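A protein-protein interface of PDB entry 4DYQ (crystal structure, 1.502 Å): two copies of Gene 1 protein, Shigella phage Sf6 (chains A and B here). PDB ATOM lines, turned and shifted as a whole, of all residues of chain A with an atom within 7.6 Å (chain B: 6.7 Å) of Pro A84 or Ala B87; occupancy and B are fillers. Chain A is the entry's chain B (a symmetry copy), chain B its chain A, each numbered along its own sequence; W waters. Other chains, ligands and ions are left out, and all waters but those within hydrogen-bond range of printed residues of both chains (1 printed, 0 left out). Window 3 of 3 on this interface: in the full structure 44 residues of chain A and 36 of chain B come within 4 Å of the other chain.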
ATOM      1  N   ASN A  81      -4.025  21.684 -19.730  1.00  0.00           N
ATOM      2  CA  ASN A  81      -4.946  21.814 -20.857  1.00  0.00           C
ATOM      3  C   ASN A  81      -5.072  23.249 -21.358  1.00  0.00           C
ATOM      4  O   ASN A  81      -5.894  23.543 -22.215  1.00  0.00           O
ATOM      5  CB  ASN A  81      -6.332  21.282 -20.477  1.00  0.00           C
ATOM      6  CG  ASN A  81      -6.326  19.794 -20.165  1.00  0.00           C
ATOM      7  OD1 ASN A  81      -5.487  19.047 -20.662  1.00  0.00           O
ATOM      8  ND2 ASN A  81      -7.265  19.360 -19.339  1.00  0.00           N
ATOM      9  N   ALA A  82      -4.257  24.154 -20.826  1.00  0.00           N
ATOM     10  CA  ALA A  82      -4.314  25.547 -21.245  1.00  0.00           C
ATOM     11  C   ALA A  82      -4.103  25.663 -22.757  1.00  0.00           C
ATOM     12  O   ALA A  82      -3.235  25.006 -23.322  1.00  0.00           O
ATOM     13  CB  ALA A  82      -3.263  26.356 -20.509  1.00  0.00           C
ATOM     14  N   ILE A  83      -4.912  26.490 -23.408  1.00  0.00           N
ATOM     15  CA  ILE A  83      -4.714  26.780 -24.824  1.00  0.00           C
ATOM     16  C   ILE A  83      -3.395  27.542 -24.960  1.00  0.00           C
ATOM     17  O   ILE A  83      -3.181  28.511 -24.245  1.00  0.00           O
ATOM     18  CB  ILE A  83      -5.861  27.645 -25.366  1.00  0.00           C
ATOM     19  CG1 ILE A  83      -7.184  26.873 -25.296  1.00  0.00           C
ATOM     20  CG2 ILE A  83      -5.563  28.098 -26.791  1.00  0.00           C
ATOM     21  CD1 ILE A  83      -8.410  27.738 -25.496  1.00  0.00           C
ATOM     22  N   PRO A  84      -2.502  27.103 -25.864  1.00  0.00           N
ATOM     23  CA  PRO A  84      -1.190  27.751 -25.990  1.00  0.00           C
ATOM     24  C   PRO A  84      -1.254  29.062 -26.768  1.00  0.00           C
ATOM     25  O   PRO A  84      -0.686  29.206 -27.850  1.00  0.00           O
ATOM     26  CB  PRO A  84      -0.344  26.705 -26.718  1.00  0.00           C
ATOM     27  CG  PRO A  84      -1.315  25.914 -27.505  1.00  0.00           C
ATOM     28  CD  PRO A  84      -2.628  25.933 -26.752  1.00  0.00           C
ATOM     29  N   ASP A  85      -1.971  30.011 -26.181  1.00  0.00           N
ATOM     30  CA  ASP A  85      -2.082  31.368 -26.672  1.00  0.00           C
ATOM     31  C   ASP A  85      -1.743  32.264 -25.491  1.00  0.00           C
ATOM     32  O   ASP A  85      -2.092  31.944 -24.359  1.00  0.00           O
ATOM     33  CB  ASP A  85      -3.506  31.618 -27.155  1.00  0.00           C
ATOM     34  CG  ASP A  85      -3.869  33.085 -27.176  1.00  0.00           C
ATOM     35  OD1 ASP A  85      -3.620  33.744 -28.207  1.00  0.00           O
ATOM     36  OD2 ASP A  85      -4.417  33.577 -26.163  1.00  0.00           O
ATOM     37  N   ALA A  86      -1.044  33.361 -25.735  1.00  0.00           N
ATOM     38  CA  ALA A  86      -0.515  34.166 -24.636  1.00  0.00           C
ATOM     39  C   ALA A  86      -1.581  34.516 -23.598  1.00  0.00           C
ATOM     40  O   ALA A  86      -1.380  34.312 -22.402  1.00  0.00           O
ATOM     41  CB  ALA A  86       0.142  35.429 -25.173  1.00  0.00           C
ATOM     42  N   ALA A  87      -2.709  35.049 -24.051  1.00  0.00           N
ATOM     43  CA  ALA A  87      -3.751  35.510 -23.142  1.00  0.00           C
ATOM     44  C   ALA A  87      -4.423  34.351 -22.413  1.00  0.00           C
ATOM     45  O   ALA A  87      -4.775  34.474 -21.239  1.00  0.00           O
ATOM     46  CB  ALA A  87      -4.785  36.329 -23.901  1.00  0.00           C
ATOM     47  N   GLU A  88      -4.608  33.231 -23.102  1.00  0.00           N
ATOM     48  CA  GLU A  88      -5.232  32.063 -22.490  1.00  0.00           C
ATOM     49  C   GLU A  88      -4.321  31.428 -21.434  1.00  0.00           C
ATOM     50  O   GLU A  88      -4.804  30.947 -20.414  1.00  0.00           O
ATOM     51  CB  GLU A  88      -5.610  31.027 -23.556  1.00  0.00           C
ATOM     52  CG  GLU A  88      -6.742  31.474 -24.497  1.00  0.00           C
ATOM     53  CD  GLU A  88      -8.130  31.417 -23.868  1.00  0.00           C
ATOM     54  OE1 GLU A  88      -8.254  31.113 -22.665  1.00  0.00           O
ATOM     55  OE2 GLU A  88      -9.114  31.684 -24.591  1.00  0.00           O
ATOM     56  N   VAL A  89      -3.015  31.403 -21.680  1.00  0.00           N
ATOM     57  CA  VAL A  89      -2.088  30.881 -20.684  1.00  0.00           C
ATOM     58  C   VAL A  89      -2.051  31.805 -19.471  1.00  0.00           C
ATOM     59  O   VAL A  89      -2.011  31.339 -18.335  1.00  0.00           O
ATOM     60  CB  VAL A  89      -0.680  30.713 -21.244  1.00  0.00           C
ATOM     61  CG1 VAL A  89       0.286  30.309 -20.131  1.00  0.00           C
ATOM     62  CG2 VAL A  89      -0.679  29.677 -22.352  1.00  0.00           C
ATOM     63  N   ALA A  90      -2.071  33.116 -19.703  1.00  0.00           N
ATOM     64  CA  ALA A  90      -2.090  34.072 -18.602  1.00  0.00           C
ATOM     65  C   ALA A  90      -3.345  33.891 -17.757  1.00  0.00           C
ATOM     66  O   ALA A  90      -3.291  33.987 -16.530  1.00  0.00           O
ATOM     67  CB  ALA A  90      -1.996  35.504 -19.132  1.00  0.00           C
ATOM     68  N   ILE B  83       8.367  23.515 -26.178  1.00  0.00           N
ATOM     69  CA  ILE B  83       8.451  24.069 -27.520  1.00  0.00           C
ATOM     70  C   ILE B  83       8.888  25.527 -27.398  1.00  0.00           C
ATOM     71  O   ILE B  83       8.304  26.284 -26.622  1.00  0.00           O
ATOM     72  CB  ILE B  83       7.094  23.968 -28.236  1.00  0.00           C
ATOM     73  CG1 ILE B  83       6.697  22.497 -28.412  1.00  0.00           C
ATOM     74  CG2 ILE B  83       7.153  24.663 -29.579  1.00  0.00           C
ATOM     75  CD1 ILE B  83       5.216  22.283 -28.678  1.00  0.00           C
ATOM     76  N   ASP B  85       8.432  28.494 -28.244  1.00  0.00           N
ATOM     77  CA  ASP B  85       7.495  29.499 -28.710  1.00  0.00           C
ATOM     78  C   ASP B  85       6.971  30.172 -27.450  1.00  0.00           C
ATOM     79  O   ASP B  85       6.824  29.521 -26.424  1.00  0.00           O
ATOM     80  CB  ASP B  85       6.372  28.825 -29.496  1.00  0.00           C
ATOM     81  CG  ASP B  85       5.100  29.640 -29.519  1.00  0.00           C
ATOM     82  OD1 ASP B  85       4.914  30.431 -30.469  1.00  0.00           O
ATOM     83  OD2 ASP B  85       4.276  29.475 -28.593  1.00  0.00           O
ATOM     84  N   ALA B  86       6.715  31.471 -27.513  1.00  0.00           N
ATOM     85  CA  ALA B  86       6.419  32.240 -26.308  1.00  0.00           C
ATOM     86  C   ALA B  86       5.308  31.614 -25.459  1.00  0.00           C
ATOM     87  O   ALA B  86       5.482  31.409 -24.258  1.00  0.00           O
ATOM     88  CB  ALA B  86       6.068  33.682 -26.672  1.00  0.00           C
ATOM     89  N   ALA B  87       4.167  31.320 -26.067  1.00  0.00           N
ATOM     90  CA  ALA B  87       3.037  30.818 -25.296  1.00  0.00           C
ATOM     91  C   ALA B  87       3.268  29.391 -24.813  1.00  0.00           C
ATOM     92  O   ALA B  87       2.815  29.023 -23.733  1.00  0.00           O
ATOM     93  CB  ALA B  87       1.767  30.897 -26.104  1.00  0.00           C
ATOM     94  N   GLU B  88       3.948  28.579 -25.613  1.00  0.00           N
ATOM     95  CA  GLU B  88       4.224  27.211 -25.204  1.00  0.00           C
ATOM     96  C   GLU B  88       5.202  27.204 -24.032  1.00  0.00           C
ATOM     97  O   GLU B  88       5.076  26.380 -23.145  1.00  0.00           O
ATOM     98  CB  GLU B  88       4.783  26.376 -26.354  1.00  0.00           C
ATOM     99  CG  GLU B  88       3.783  26.071 -27.478  1.00  0.00           C
ATOM    100  CD  GLU B  88       2.747  25.007 -27.120  1.00  0.00           C
ATOM    101  OE1 GLU B  88       2.727  24.520 -25.970  1.00  0.00           O
ATOM    102  OE2 GLU B  88       1.936  24.652 -28.000  1.00  0.00           O
ATOM    103  N   VAL B  89       6.175  28.114 -24.024  1.00  0.00           N
ATOM    104  CA  VAL B  89       7.101  28.182 -22.895  1.00  0.00           C
ATOM    105  C   VAL B  89       6.363  28.672 -21.654  1.00  0.00           C
ATOM    106  O   VAL B  89       6.587  28.158 -20.557  1.00  0.00           O
ATOM    107  CB  VAL B  89       8.328  29.070 -23.183  1.00  0.00           C
ATOM    108  CG1 VAL B  89       9.167  29.232 -21.917  1.00  0.00           C
ATOM    109  CG2 VAL B  89       9.155  28.471 -24.299  1.00  0.00           C
ATOM    110  N   ALA B  90       5.471  29.650 -21.811  1.00  0.00           N
ATOM    111  CA  ALA B  90       4.673  30.118 -20.679  1.00  0.00           C
ATOM    112  C   ALA B  90       3.793  28.999 -20.126  1.00  0.00           C
ATOM    113  O   ALA B  90       3.623  28.876 -18.913  1.00  0.00           O
ATOM    114  CB  ALA B  90       3.815  31.311 -21.077  1.00  0.00           C
ATOM    115  N   LYS B  91       3.230  28.185 -21.010  1.00  0.00           N
ATOM    116  CA  LYS B  91       2.430  27.047 -20.572  1.00  0.00           C
ATOM    117  C   LYS B  91       3.283  26.022 -19.832  1.00  0.00           C
ATOM    118  O   LYS B  91       2.879  25.510 -18.790  1.00  0.00           O
ATOM    119  CB  LYS B  91       1.730  26.387 -21.763  1.00  0.00           C
ATOM    120  CG  LYS B  91       0.962  25.147 -21.372  1.00  0.00           C
ATOM    121  CD  LYS B  91       0.105  24.618 -22.514  1.00  0.00           C
ATOM    122  CE  LYS B  91      -0.534  23.295 -22.133  1.00  0.00           C
ATOM    123  NZ  LYS B  91      -1.462  22.803 -23.193  1.00  0.00           N
ATOM    124  N   ALA B  92       4.452  25.705 -20.378  1.00  0.00           N
ATOM    125  CA  ALA B  92       5.367  24.776 -19.718  1.00  0.00           C
ATOM    126  C   ALA B  92       5.736  25.288 -18.330  1.00  0.00           C
ATOM    127  O   ALA B  92       5.788  24.510 -17.383  1.00  0.00           O
ATOM    128  CB  ALA B  92       6.602  24.573 -20.554  1.00  0.00           C
HETATM  129  O   HOH W   1       1.638  28.957 -29.385  1.00  0.00           O
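OD2 of Asp B85 lies within hydrogen-bond range of N of Ala B87, 3.1 Å away.
OD2 of Asp B85 is in hydrogen-bond range of N of Glu B88.
The side-chain carboxylate (OD2) of Asp A85 sits at hydrogen-bond distance from the backbone NH (N) of Ala A87 (3.1 Å).
OD2 of Asp A85 lies within hydrogen-bond range of N of Glu A88, 3.1 Å away.
Asp A85 touches Ala B87, but with the chains exchanged Ala A87 does not touch Asp B85 (10.0 Å).
Ala A86 touches Ala B87, but with the chains exchanged Ala A87 does not touch Ala B86 (8.8 Å).
Val A89 touches Ala B87, but with the chains exchanged Ala A87 does not touch Val B89 (11.3 Å).
Val A89 touches Ala B90, but with the chains exchanged Ala A90 does not touch Val B89 (9.7 Å).
Positions printed for both chains: 83, 85, 86, 87, 88, 89 and 90.
Water W1 lies within hydrogen-bond range of the backbone carbonyl oxygen (O) of Pro A84 and the side-chain carboxylate (OD2) of Asp B85.
NZ of Lys B91 is in hydrogen-bond range of O of Ala A82 (2.8 Å).
Pro A84 touches Ala B87.
CB of Pro A84 touches OE2 of Glu B88 (3.3 Å).
Asp A85 touches Ala B87.
CB of Ala B87 touches N of Ala A86, 3.8 Å away.
Ala B87 touches Val A89 (O to CG2, 3.8 Å).
Val A89 touches Ala B90 (CG1 to C, 3.7 Å).
Val A89 touches Lys B91.
Pro A84 touches just these residues of chain B: Ala B87 and Glu B88.
Printed residues of chain A within 4 Å of Ala B87: Pro A84, Asp A85, Ala A86 and Val A89.
No residue of chain A comes within 4 Å of Ala B86.
Of the printed residues of chain B, Val A89 touches Ala B87, Ala B90 and Lys B91.
Printed residues of chain A within 4 Å of Glu B88: Pro A84 (3.3 Å).
Of the printed residues of chain B, Ala A82 touches Lys B91.
Of the printed residues of chain A, Lys B91 touches Ala A82 (2.8 Å) and Val A89 (3.7 Å).
Of the printed residues of chain B, Asp A85 touches Ala B87 (3.8 Å).
Glu A88 touches none of the printed residues of chain B.
The nearest residue of chain B that does not touch Pro A84 is Lys B91 (4.7 Å).
Hydrophobic or aromatic side chains of chain B that line the printed part of chain A: Ala B87 and Ala B90.
Among the printed residues, no Asp or Glu carboxylate lies within 4 Å of a Lys or Arg side-chain nitrogen of the other chain.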
